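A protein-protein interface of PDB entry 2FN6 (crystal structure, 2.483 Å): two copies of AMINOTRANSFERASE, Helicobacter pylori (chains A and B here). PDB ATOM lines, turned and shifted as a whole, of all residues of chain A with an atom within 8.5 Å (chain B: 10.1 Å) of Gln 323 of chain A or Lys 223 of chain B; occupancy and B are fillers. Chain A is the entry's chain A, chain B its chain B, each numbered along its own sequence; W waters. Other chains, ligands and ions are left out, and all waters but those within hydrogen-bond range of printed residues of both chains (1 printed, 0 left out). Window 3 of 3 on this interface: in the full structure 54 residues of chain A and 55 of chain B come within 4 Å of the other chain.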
ATOM      1  N   VAL A  85      28.711  19.788  27.939  1.00  0.00           N
ATOM      2  CA  VAL A  85      27.580  19.172  28.658  1.00  0.00           C
ATOM      3  C   VAL A  85      27.349  19.762  30.059  1.00  0.00           C
ATOM      4  O   VAL A  85      26.230  19.713  30.588  1.00  0.00           O
ATOM      5  CB  VAL A  85      27.706  17.613  28.715  1.00  0.00           C
ATOM      6  CG1 VAL A  85      28.888  17.182  29.591  1.00  0.00           C
ATOM      7  CG2 VAL A  85      26.428  16.966  29.227  1.00  0.00           C
ATOM      8  N   ASN A  89      24.230  19.877  32.629  1.00  0.00           N
ATOM      9  CA  ASN A  89      24.288  18.930  33.751  1.00  0.00           C
ATOM     10  C   ASN A  89      24.007  19.627  35.066  1.00  0.00           C
ATOM     11  O   ASN A  89      23.361  19.076  35.952  1.00  0.00           O
ATOM     12  CB  ASN A  89      25.660  18.245  33.830  1.00  0.00           C
ATOM     13  CG  ASN A  89      25.784  17.028  32.912  1.00  0.00           C
ATOM     14  OD1 ASN A  89      24.868  16.692  32.174  1.00  0.00           O
ATOM     15  ND2 ASN A  89      26.936  16.359  32.967  1.00  0.00           N
ATOM     16  N   LYS A 317      28.997  18.339  20.347  1.00  0.00           N
ATOM     17  CA  LYS A 317      27.878  17.422  20.200  1.00  0.00           C
ATOM     18  C   LYS A 317      26.621  18.052  20.839  1.00  0.00           C
ATOM     19  O   LYS A 317      26.649  18.445  22.007  1.00  0.00           O
ATOM     20  CB  LYS A 317      28.252  16.100  20.871  1.00  0.00           C
ATOM     21  CG  LYS A 317      27.116  15.327  21.510  1.00  0.00           C
ATOM     22  CD  LYS A 317      26.588  14.249  20.608  1.00  0.00           C
ATOM     23  CE  LYS A 317      27.476  13.013  20.607  1.00  0.00           C
ATOM     24  NZ  LYS A 317      27.325  12.235  21.836  1.00  0.00           N
ATOM     25  N   PRO A 318      25.517  18.166  20.077  1.00  0.00           N
ATOM     26  CA  PRO A 318      24.343  18.772  20.680  1.00  0.00           C
ATOM     27  C   PRO A 318      23.987  18.051  21.959  1.00  0.00           C
ATOM     28  O   PRO A 318      23.927  16.829  21.968  1.00  0.00           O
ATOM     29  CB  PRO A 318      23.266  18.566  19.616  1.00  0.00           C
ATOM     30  CG  PRO A 318      24.033  18.561  18.339  1.00  0.00           C
ATOM     31  CD  PRO A 318      25.267  17.783  18.677  1.00  0.00           C
ATOM     32  N   ILE A 319      23.769  18.802  23.032  1.00  0.00           N
ATOM     33  CA  ILE A 319      23.605  18.194  24.359  1.00  0.00           C
ATOM     34  C   ILE A 319      22.462  17.182  24.464  1.00  0.00           C
ATOM     35  O   ILE A 319      22.603  16.156  25.136  1.00  0.00           O
ATOM     36  CB  ILE A 319      23.516  19.247  25.474  1.00  0.00           C
ATOM     37  CG1 ILE A 319      24.877  19.923  25.643  1.00  0.00           C
ATOM     38  CG2 ILE A 319      23.094  18.604  26.789  1.00  0.00           C
ATOM     39  CD1 ILE A 319      24.895  21.087  26.648  1.00  0.00           C
ATOM     40  N   TYR A 320      21.351  17.463  23.785  1.00  0.00           N
ATOM     41  CA  TYR A 320      20.142  16.627  23.879  1.00  0.00           C
ATOM     42  C   TYR A 320      20.373  15.253  23.278  1.00  0.00           C
ATOM     43  O   TYR A 320      19.559  14.356  23.491  1.00  0.00           O
ATOM     44  CB  TYR A 320      18.920  17.298  23.214  1.00  0.00           C
ATOM     45  CG  TYR A 320      19.139  17.671  21.765  1.00  0.00           C
ATOM     46  CD1 TYR A 320      19.433  18.982  21.406  1.00  0.00           C
ATOM     47  CD2 TYR A 320      19.072  16.706  20.752  1.00  0.00           C
ATOM     48  CE1 TYR A 320      19.649  19.328  20.080  1.00  0.00           C
ATOM     49  CE2 TYR A 320      19.292  17.037  19.412  1.00  0.00           C
ATOM     50  CZ  TYR A 320      19.576  18.350  19.089  1.00  0.00           C
ATOM     51  OH  TYR A 320      19.809  18.696  17.783  1.00  0.00           O
ATOM     52  N   GLN A 321      21.477  15.109  22.533  1.00  0.00           N
ATOM     53  CA  GLN A 321      21.867  13.851  21.877  1.00  0.00           C
ATOM     54  C   GLN A 321      22.439  12.791  22.823  1.00  0.00           C
ATOM     55  O   GLN A 321      22.422  11.600  22.492  1.00  0.00           O
ATOM     56  CB  GLN A 321      22.892  14.100  20.769  1.00  0.00           C
ATOM     57  CG  GLN A 321      22.308  14.560  19.453  1.00  0.00           C
ATOM     58  CD  GLN A 321      23.244  14.321  18.275  1.00  0.00           C
ATOM     59  OE1 GLN A 321      24.360  13.806  18.430  1.00  0.00           O
ATOM     60  NE2 GLN A 321      22.783  14.684  17.081  1.00  0.00           N
ATOM     61  N   TYR A 322      22.970  13.206  23.976  1.00  0.00           N
ATOM     62  CA  TYR A 322      23.478  12.238  24.943  1.00  0.00           C
ATOM     63  C   TYR A 322      22.348  11.377  25.488  1.00  0.00           C
ATOM     64  O   TYR A 322      21.206  11.838  25.580  1.00  0.00           O
ATOM     65  CB  TYR A 322      24.177  12.936  26.102  1.00  0.00           C
ATOM     66  CG  TYR A 322      25.487  13.567  25.749  1.00  0.00           C
ATOM     67  CD1 TYR A 322      26.558  12.793  25.290  1.00  0.00           C
ATOM     68  CD2 TYR A 322      25.672  14.944  25.890  1.00  0.00           C
ATOM     69  CE1 TYR A 322      27.780  13.375  24.967  1.00  0.00           C
ATOM     70  CE2 TYR A 322      26.881  15.540  25.572  1.00  0.00           C
ATOM     71  CZ  TYR A 322      27.942  14.756  25.115  1.00  0.00           C
ATOM     72  OH  TYR A 322      29.153  15.352  24.808  1.00  0.00           O
ATOM     73  N   GLN A 323      22.686  10.143  25.864  1.00  0.00           N
ATOM     74  CA  GLN A 323      21.746   9.172  26.440  1.00  0.00           C
ATOM     75  C   GLN A 323      20.911   9.733  27.572  1.00  0.00           C
ATOM     76  O   GLN A 323      19.703   9.513  27.628  1.00  0.00           O
ATOM     77  CB  GLN A 323      22.486   7.942  26.967  1.00  0.00           C
ATOM     78  CG  GLN A 323      22.390   6.717  26.084  1.00  0.00           C
ATOM     79  CD  GLN A 323      22.447   5.428  26.888  1.00  0.00           C
ATOM     80  OE1 GLN A 323      21.885   5.333  27.988  1.00  0.00           O
ATOM     81  NE2 GLN A 323      23.122   4.428  26.340  1.00  0.00           N
ATOM     82  N   LEU A 324      21.563  10.448  28.477  1.00  0.00           N
ATOM     83  CA  LEU A 324      20.896  11.003  29.643  1.00  0.00           C
ATOM     84  C   LEU A 324      19.735  11.889  29.222  1.00  0.00           C
ATOM     85  O   LEU A 324      18.657  11.826  29.811  1.00  0.00           O
ATOM     86  CB  LEU A 324      21.890  11.834  30.447  1.00  0.00           C
ATOM     87  CG  LEU A 324      21.743  12.050  31.951  1.00  0.00           C
ATOM     88  CD1 LEU A 324      22.341  13.407  32.309  1.00  0.00           C
ATOM     89  CD2 LEU A 324      20.327  11.921  32.465  1.00  0.00           C
ATOM     90  N   TYR A 325      19.964  12.714  28.201  1.00  0.00           N
ATOM     91  CA  TYR A 325      18.977  13.700  27.775  1.00  0.00           C
ATOM     92  C   TYR A 325      17.857  13.079  26.937  1.00  0.00           C
ATOM     93  O   TYR A 325      16.700  13.506  27.024  1.00  0.00           O
ATOM     94  CB  TYR A 325      19.669  14.887  27.092  1.00  0.00           C
ATOM     95  CG  TYR A 325      20.492  15.667  28.094  1.00  0.00           C
ATOM     96  CD1 TYR A 325      21.803  15.286  28.407  1.00  0.00           C
ATOM     97  CD2 TYR A 325      19.936  16.736  28.788  1.00  0.00           C
ATOM     98  CE1 TYR A 325      22.539  15.968  29.358  1.00  0.00           C
ATOM     99  CE2 TYR A 325      20.664  17.423  29.732  1.00  0.00           C
ATOM    100  CZ  TYR A 325      21.969  17.037  30.013  1.00  0.00           C
ATOM    101  OH  TYR A 325      22.681  17.732  30.954  1.00  0.00           O
ATOM    102  N   GLN A 326      18.206  12.048  26.167  1.00  0.00           N
ATOM    103  CA  GLN A 326      17.236  11.273  25.399  1.00  0.00           C
ATOM    104  C   GLN A 326      16.338  10.397  26.275  1.00  0.00           C
ATOM    105  O   GLN A 326      15.223  10.060  25.869  1.00  0.00           O
ATOM    106  CB  GLN A 326      17.928  10.430  24.321  1.00  0.00           C
ATOM    107  CG  GLN A 326      18.292  11.204  23.057  1.00  0.00           C
ATOM    108  CD  GLN A 326      17.089  11.925  22.434  1.00  0.00           C
ATOM    109  OE1 GLN A 326      16.015  11.335  22.270  1.00  0.00           O
ATOM    110  NE2 GLN A 326      17.264  13.203  22.092  1.00  0.00           N
ATOM    111  N   GLN A 327      16.814  10.033  27.464  1.00  0.00           N
ATOM    112  CA  GLN A 327      15.992   9.273  28.410  1.00  0.00           C
ATOM    113  C   GLN A 327      15.039  10.198  29.162  1.00  0.00           C
ATOM    114  O   GLN A 327      13.890   9.847  29.391  1.00  0.00           O
ATOM    115  CB  GLN A 327      16.836   8.466  29.422  1.00  0.00           C
ATOM    116  CG  GLN A 327      17.966   7.596  28.840  1.00  0.00           C
ATOM    117  CD  GLN A 327      17.534   6.206  28.368  1.00  0.00           C
ATOM    118  OE1 GLN A 327      18.312   5.251  28.449  1.00  0.00           O
ATOM    119  NE2 GLN A 327      16.308   6.092  27.856  1.00  0.00           N
ATOM    120  N   LEU A 328      15.520  11.372  29.549  1.00  0.00           N
ATOM    121  CA  LEU A 328      14.732  12.280  30.368  1.00  0.00           C
ATOM    122  C   LEU A 328      13.737  13.114  29.571  1.00  0.00           C
ATOM    123  O   LEU A 328      12.633  13.374  30.045  1.00  0.00           O
ATOM    124  CB  LEU A 328      15.629  13.210  31.188  1.00  0.00           C
ATOM    125  CG  LEU A 328      16.545  12.675  32.299  1.00  0.00           C
ATOM    126  CD1 LEU A 328      16.931  13.822  33.231  1.00  0.00           C
ATOM    127  CD2 LEU A 328      15.935  11.532  33.107  1.00  0.00           C
ATOM    128  N   PHE A 329      14.133  13.547  28.379  1.00  0.00           N
ATOM    129  CA  PHE A 329      13.353  14.532  27.639  1.00  0.00           C
ATOM    130  C   PHE A 329      12.992  14.095  26.231  1.00  0.00           C
ATOM    131  O   PHE A 329      12.101  14.681  25.617  1.00  0.00           O
ATOM    132  CB  PHE A 329      14.095  15.871  27.578  1.00  0.00           C
ATOM    133  CG  PHE A 329      14.561  16.364  28.915  1.00  0.00           C
ATOM    134  CD1 PHE A 329      15.919  16.463  29.196  1.00  0.00           C
ATOM    135  CD2 PHE A 329      13.645  16.708  29.900  1.00  0.00           C
ATOM    136  CE1 PHE A 329      16.363  16.915  30.443  1.00  0.00           C
ATOM    137  CE2 PHE A 329      14.074  17.154  31.148  1.00  0.00           C
ATOM    138  CZ  PHE A 329      15.438  17.259  31.421  1.00  0.00           C
ATOM    139  N   ASN A 330      13.684  13.078  25.717  1.00  0.00           N
ATOM    140  CA  ASN A 330      13.450  12.608  24.356  1.00  0.00           C
ATOM    141  C   ASN A 330      13.218  13.788  23.384  1.00  0.00           C
ATOM    142  O   ASN A 330      12.169  13.899  22.747  1.00  0.00           O
ATOM    143  CB  ASN A 330      12.286  11.602  24.344  1.00  0.00           C
ATOM    144  CG  ASN A 330      11.863  11.202  22.945  1.00  0.00           C
ATOM    145  OD1 ASN A 330      10.674  11.208  22.629  1.00  0.00           O
ATOM    146  ND2 ASN A 330      12.832  10.869  22.090  1.00  0.00           N
ATOM    147  N   GLU B  69      21.753   4.035  45.312  1.00  0.00           N
ATOM    148  CA  GLU B  69      20.687   4.894  44.816  1.00  0.00           C
ATOM    149  C   GLU B  69      19.829   5.353  45.988  1.00  0.00           C
ATOM    150  O   GLU B  69      19.601   4.590  46.928  1.00  0.00           O
ATOM    151  CB  GLU B  69      19.848   4.177  43.754  1.00  0.00           C
ATOM    152  CG  GLU B  69      20.419   4.282  42.340  1.00  0.00           C
ATOM    153  CD  GLU B  69      20.419   5.723  41.761  1.00  0.00           C
ATOM    154  OE1 GLU B  69      20.245   6.726  42.506  1.00  0.00           O
ATOM    155  OE2 GLU B  69      20.612   5.847  40.534  1.00  0.00           O
ATOM    156  N   LYS B 203      31.812   4.327  39.318  1.00  0.00           N
ATOM    157  CA  LYS B 203      30.637   5.190  39.383  1.00  0.00           C
ATOM    158  C   LYS B 203      31.035   6.561  39.931  1.00  0.00           C
ATOM    159  O   LYS B 203      30.550   7.594  39.453  1.00  0.00           O
ATOM    160  CB  LYS B 203      29.599   4.547  40.301  1.00  0.00           C
ATOM    161  CG  LYS B 203      28.169   4.595  39.826  1.00  0.00           C
ATOM    162  CD  LYS B 203      27.209   4.078  40.917  1.00  0.00           C
ATOM    163  CE  LYS B 203      25.915   4.900  40.894  1.00  0.00           C
ATOM    164  NZ  LYS B 203      25.046   4.730  42.103  1.00  0.00           N
ATOM    165  N   LEU B 206      33.071   8.607  37.379  1.00  0.00           N
ATOM    166  CA  LEU B 206      32.179   9.312  36.439  1.00  0.00           C
ATOM    167  C   LEU B 206      31.557  10.570  37.049  1.00  0.00           C
ATOM    168  O   LEU B 206      31.482  11.604  36.401  1.00  0.00           O
ATOM    169  CB  LEU B 206      31.088   8.377  35.883  1.00  0.00           C
ATOM    170  CG  LEU B 206      31.608   7.248  34.971  1.00  0.00           C
ATOM    171  CD1 LEU B 206      30.486   6.286  34.608  1.00  0.00           C
ATOM    172  CD2 LEU B 206      32.327   7.779  33.711  1.00  0.00           C
ATOM    173  N   PHE B 207      31.139  10.477  38.302  1.00  0.00           N
ATOM    174  CA  PHE B 207      30.559  11.596  39.013  1.00  0.00           C
ATOM    175  C   PHE B 207      31.565  12.751  39.179  1.00  0.00           C
ATOM    176  O   PHE B 207      31.183  13.932  39.217  1.00  0.00           O
ATOM    177  CB  PHE B 207      30.086  11.111  40.385  1.00  0.00           C
ATOM    178  CG  PHE B 207      29.145  12.055  41.078  1.00  0.00           C
ATOM    179  CD1 PHE B 207      29.608  12.924  42.048  1.00  0.00           C
ATOM    180  CD2 PHE B 207      27.789  12.057  40.767  1.00  0.00           C
ATOM    181  CE1 PHE B 207      28.737  13.786  42.695  1.00  0.00           C
ATOM    182  CE2 PHE B 207      26.911  12.913  41.405  1.00  0.00           C
ATOM    183  CZ  PHE B 207      27.383  13.781  42.369  1.00  0.00           C
ATOM    184  N   SER B 209      33.760  13.675  37.047  1.00  0.00           N
ATOM    185  CA  SER B 209      34.051  14.358  35.800  1.00  0.00           C
ATOM    186  C   SER B 209      32.915  14.274  34.781  1.00  0.00           C
ATOM    187  O   SER B 209      33.005  13.517  33.812  1.00  0.00           O
ATOM    188  CB  SER B 209      35.385  13.864  35.213  1.00  0.00           C
ATOM    189  OG  SER B 209      35.866  14.741  34.198  1.00  0.00           O
ATOM    190  N   HIS B 210      31.843  15.044  35.017  1.00  0.00           N
ATOM    191  CA  HIS B 210      30.773  15.285  34.027  1.00  0.00           C
ATOM    192  C   HIS B 210      29.965  14.060  33.582  1.00  0.00           C
ATOM    193  O   HIS B 210      29.094  14.194  32.715  1.00  0.00           O
ATOM    194  CB  HIS B 210      31.339  15.965  32.763  1.00  0.00           C
ATOM    195  CG  HIS B 210      32.236  17.120  33.049  1.00  0.00           C
ATOM    196  ND1 HIS B 210      31.796  18.265  33.681  1.00  0.00           N
ATOM    197  CD2 HIS B 210      33.555  17.307  32.801  1.00  0.00           C
ATOM    198  CE1 HIS B 210      32.806  19.107  33.810  1.00  0.00           C
ATOM    199  NE2 HIS B 210      33.882  18.555  33.274  1.00  0.00           N
ATOM    200  N   GLY B 211      30.258  12.881  34.143  1.00  0.00           N
ATOM    201  CA  GLY B 211      29.678  11.627  33.676  1.00  0.00           C
ATOM    202  C   GLY B 211      30.134  11.247  32.278  1.00  0.00           C
ATOM    203  O   GLY B 211      29.570  10.352  31.673  1.00  0.00           O
ATOM    204  N   MET B 212      31.158  11.921  31.761  1.00  0.00           N
ATOM    205  CA  MET B 212      31.670  11.655  30.413  1.00  0.00           C
ATOM    206  C   MET B 212      32.341  10.287  30.274  1.00  0.00           C
ATOM    207  O   MET B 212      33.318   9.998  30.957  1.00  0.00           O
ATOM    208  CB  MET B 212      32.646  12.770  29.982  1.00  0.00           C
ATOM    209  CG  MET B 212      33.067  12.755  28.493  1.00  0.00           C
ATOM    210  SD  MET B 212      31.696  13.051  27.335  1.00  0.00           S
ATOM    211  CE  MET B 212      31.352  14.759  27.716  1.00  0.00           C
ATOM    212  N   LEU B 213      31.807   9.459  29.384  1.00  0.00           N
ATOM    213  CA  LEU B 213      32.410   8.179  29.016  1.00  0.00           C
ATOM    214  C   LEU B 213      33.172   8.363  27.712  1.00  0.00           C
ATOM    215  O   LEU B 213      32.618   8.868  26.744  1.00  0.00           O
ATOM    216  CB  LEU B 213      31.323   7.127  28.798  1.00  0.00           C
ATOM    217  CG  LEU B 213      30.369   6.775  29.938  1.00  0.00           C
ATOM    218  CD1 LEU B 213      28.990   6.389  29.395  1.00  0.00           C
ATOM    219  CD2 LEU B 213      30.955   5.637  30.780  1.00  0.00           C
ATOM    220  N   LYS B 214      34.434   7.952  27.675  1.00  0.00           N
ATOM    221  CA  LYS B 214      35.226   8.066  26.442  1.00  0.00           C
ATOM    222  C   LYS B 214      34.807   7.021  25.395  1.00  0.00           C
ATOM    223  O   LYS B 214      34.818   5.822  25.677  1.00  0.00           O
ATOM    224  CB  LYS B 214      36.734   7.970  26.748  1.00  0.00           C
ATOM    225  CG  LYS B 214      37.668   8.438  25.609  1.00  0.00           C
ATOM    226  CD  LYS B 214      37.798   9.973  25.510  1.00  0.00           C
ATOM    227  CE  LYS B 214      36.509  10.654  24.998  1.00  0.00           C
ATOM    228  NZ  LYS B 214      36.725  12.053  24.514  1.00  0.00           N
ATOM    229  N   LYS B 215      34.421   7.479  24.202  1.00  0.00           N
ATOM    230  CA  LYS B 215      34.081   6.580  23.084  1.00  0.00           C
ATOM    231  C   LYS B 215      35.282   6.430  22.136  1.00  0.00           C
ATOM    232  O   LYS B 215      36.061   5.489  22.271  1.00  0.00           O
ATOM    233  CB  LYS B 215      32.826   7.065  22.353  1.00  0.00           C
ATOM    234  CG  LYS B 215      32.183   6.023  21.444  1.00  0.00           C
ATOM    235  CD  LYS B 215      30.748   6.413  21.074  1.00  0.00           C
ATOM    236  CE  LYS B 215      29.762   6.143  22.219  1.00  0.00           C
ATOM    237  NZ  LYS B 215      28.362   6.552  21.882  1.00  0.00           N
ATOM    238  N   GLU B 219      34.414  11.908  20.364  1.00  0.00           N
ATOM    239  CA  GLU B 219      33.067  11.803  20.910  1.00  0.00           C
ATOM    240  C   GLU B 219      33.063  11.012  22.204  1.00  0.00           C
ATOM    241  O   GLU B 219      33.921  10.168  22.429  1.00  0.00           O
ATOM    242  CB  GLU B 219      32.133  11.159  19.878  1.00  0.00           C
ATOM    243  CG  GLU B 219      30.655  11.091  20.278  1.00  0.00           C
ATOM    244  CD  GLU B 219      29.792  10.352  19.254  1.00  0.00           C
ATOM    245  OE1 GLU B 219      28.554  10.301  19.449  1.00  0.00           O
ATOM    246  OE2 GLU B 219      30.346   9.827  18.255  1.00  0.00           O
ATOM    247  N   GLY B 220      32.092  11.308  23.054  1.00  0.00           N
ATOM    248  CA  GLY B 220      31.831  10.527  24.250  1.00  0.00           C
ATOM    249  C   GLY B 220      30.342  10.351  24.478  1.00  0.00           C
ATOM    250  O   GLY B 220      29.524  10.843  23.703  1.00  0.00           O
ATOM    251  N   GLU B 221      29.998   9.657  25.553  1.00  0.00           N
ATOM    252  CA  GLU B 221      28.614   9.454  25.938  1.00  0.00           C
ATOM    253  C   GLU B 221      28.419   9.879  27.396  1.00  0.00           C
ATOM    254  O   GLU B 221      29.331   9.752  28.224  1.00  0.00           O
ATOM    255  CB  GLU B 221      28.251   7.980  25.752  1.00  0.00           C
ATOM    256  CG  GLU B 221      26.784   7.643  25.964  1.00  0.00           C
ATOM    257  CD  GLU B 221      25.860   8.350  24.983  1.00  0.00           C
ATOM    258  OE1 GLU B 221      25.860   7.999  23.787  1.00  0.00           O
ATOM    259  OE2 GLU B 221      25.123   9.256  25.413  1.00  0.00           O
ATOM    260  N   VAL B 222      27.238  10.408  27.703  1.00  0.00           N
ATOM    261  CA  VAL B 222      26.879  10.747  29.080  1.00  0.00           C
ATOM    262  C   VAL B 222      25.592  10.002  29.411  1.00  0.00           C
ATOM    263  O   VAL B 222      24.611  10.120  28.682  1.00  0.00           O
ATOM    264  CB  VAL B 222      26.684  12.280  29.261  1.00  0.00           C
ATOM    265  CG1 VAL B 222      26.472  12.633  30.732  1.00  0.00           C
ATOM    266  CG2 VAL B 222      27.882  13.074  28.694  1.00  0.00           C
ATOM    267  N   LYS B 223      25.601   9.232  30.498  1.00  0.00           N
ATOM    268  CA  LYS B 223      24.439   8.430  30.908  1.00  0.00           C
ATOM    269  C   LYS B 223      23.914   8.816  32.262  1.00  0.00           C
ATOM    270  O   LYS B 223      22.874   8.333  32.690  1.00  0.00           O
ATOM    271  CB  LYS B 223      24.784   6.945  30.956  1.00  0.00           C
ATOM    272  CG  LYS B 223      24.672   6.263  29.625  1.00  0.00           C
ATOM    273  CD  LYS B 223      25.223   4.871  29.673  1.00  0.00           C
ATOM    274  CE  LYS B 223      25.825   4.521  28.329  1.00  0.00           C
ATOM    275  NZ  LYS B 223      26.571   3.253  28.447  1.00  0.00           N
ATOM    276  N   SER B 224      24.665   9.666  32.947  1.00  0.00           N
ATOM    277  CA  SER B 224      24.343  10.119  34.292  1.00  0.00           C
ATOM    278  C   SER B 224      25.102  11.418  34.513  1.00  0.00           C
ATOM    279  O   SER B 224      26.133  11.653  33.872  1.00  0.00           O
ATOM    280  CB  SER B 224      24.823   9.084  35.285  1.00  0.00           C
ATOM    281  OG  SER B 224      26.087   8.598  34.858  1.00  0.00           O
ATOM    282  N   ILE B 225      24.611  12.277  35.394  1.00  0.00           N
ATOM    283  CA  ILE B 225      25.292  13.552  35.573  1.00  0.00           C
ATOM    284  C   ILE B 225      26.628  13.339  36.290  1.00  0.00           C
ATOM    285  O   ILE B 225      26.908  12.275  36.862  1.00  0.00           O
ATOM    286  CB  ILE B 225      24.436  14.650  36.316  1.00  0.00           C
ATOM    287  CG1 ILE B 225      23.982  14.167  37.686  1.00  0.00           C
ATOM    288  CG2 ILE B 225      23.274  15.133  35.478  1.00  0.00           C
ATOM    289  CD1 ILE B 225      25.040  14.385  38.746  1.00  0.00           C
ATOM    290  N   GLY B 226      27.455  14.363  36.225  1.00  0.00           N
ATOM    291  CA  GLY B 226      28.667  14.410  36.991  1.00  0.00           C
ATOM    292  C   GLY B 226      29.041  15.860  37.099  1.00  0.00           C
ATOM    293  O   GLY B 226      28.423  16.723  36.455  1.00  0.00           O
HETATM  294  O   HOH W   1      28.905  18.362  34.149  1.00  0.00           O
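OE1 of Glu 219 of chain B is in salt-bridge range of NZ of Lys 317 of chain A (3.3 Å). O of His 210 of chain B lies within hydrogen-bond range of ND2 of Asn 89 of chain A, at 3.1 Å. The backbone carbonyl oxygen (O) of Val 222 of chain B is in hydrogen-bond range of the backbone NH (N) of Gln 323 of chain A. N of Gln 323 of chain A is in hydrogen-bond range of OE2 of Glu 221 of chain B, 2.6 Å away. The backbone NH (N) of Leu 324 of chain A sits at hydrogen-bond distance from the backbone carbonyl oxygen (O) of Val 222 of chain B (3.1 Å). The side-chain amino group (NZ) of Lys 317 of chain A lies within hydrogen-bond range of the backbone carbonyl oxygen (O) of Gly 220 of chain B (3.2 Å).
OE1 of Glu 221 of chain B is in salt-bridge range of NZ of Lys 215 of chain B. The backbone NH (N) of Leu 213 of chain B is in hydrogen-bond range of the backbone carbonyl oxygen (O) of Glu 221 of chain B (2.7 Å). OD1 of Asn 89 of chain A lies within hydrogen-bond range of OH of Tyr 325 of chain A, at 2.7 Å.
Ile 225 of chain B touches Asn 89 of chain A (CG2 to O, 3.97 Å). ND2 of Asn 89 of chain A touches O of Gly 226 of chain B, 3.8 Å away. Tyr 322 of chain A touches Met 212 of chain B. O of Gly 220 of chain B touches CE1 of Tyr 322 of chain A, at 3.3 Å. Tyr 322 of chain A touches Glu 221 of chain B (CA to OE2, 3.4 Å). CD1 of Tyr 322 of chain A touches N of Val 222 of chain B, 3.5 Å away. Gln 323 of chain A touches Lys 223 of chain B (NE2 to CE, 3.4 Å). CG of Leu 324 of chain A touches C of Lys 223 of chain B (3.9 Å). Leu 324 of chain A touches Ser 224 of chain B (CG to N, 3.9 Å). CD1 of Leu 324 of chain A touches CG2 of Ile 225 of chain B (3.7 Å).
Tyr 320 of chain A touches none of the printed residues of chain B. Printed residues of chain B within 4 Å of Tyr 322 of chain A: Met 212 (3.7 Å), Gly 220 (3.3 Å), Glu 221 (3.4 Å) and Val 222 (3.5 Å). Leu 324 of chain A touches just these residues of chain B: Val 222 (3.1 Å), Lys 223 (3.9 Å), Ser 224 (3.9 Å) and Ile 225 (3.7 Å). Of the printed residues of chain A, Glu 219 of chain B touches Lys 317. Of the printed residues of chain A, Glu 221 of chain B touches Tyr 322 (3.4 Å) and Gln 323 (2.6 Å). Printed residues of chain A within 4 Å of Val 222 of chain B: Tyr 322, Gln 323 and Leu 324. Of chain A, only Gln 323 and Leu 324 come within 4 Å of Lys 223 of chain B. The nearest residue of chain B that does not touch Gln 323 of chain A is Ser 224 of chain B (6.6 Å). The nearest residue of chain A that does not touch Lys 223 of chain B is Tyr 322 of chain A (5.9 Å). The nearest printed residue of chain A that does not touch Val 222 of chain B is Val 85 of chain A (4.2 Å).
Hydrophobic or aromatic side chains of chain B within 4 Å of the printed part of chain A: Met 212, Val 222 and Ile 225. Printed residues of chain A that touch a printed residue of chain B: Val 85, Asn 89, Lys 317, Tyr 322, Gln 323 and Leu 324. Among the printed residues, Asp or Glu carboxylates within 4 Å of a Lys or Arg side-chain nitrogen of the other chain: Lys 317 of chain A with Glu 219 of chain B (3.3 Å).
No position is printed for both chains. Of the 17 pairs that touch across the chains among the printed residues, none has its exchanged pair printed and touching as well.
Water W1 lies within hydrogen-bond range of O of Gly 226 of chain B (2.9 Å), ND1 of His 210 of chain B (2.9 Å) and ND2 of Asn 89 of chain A (3.0 Å).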
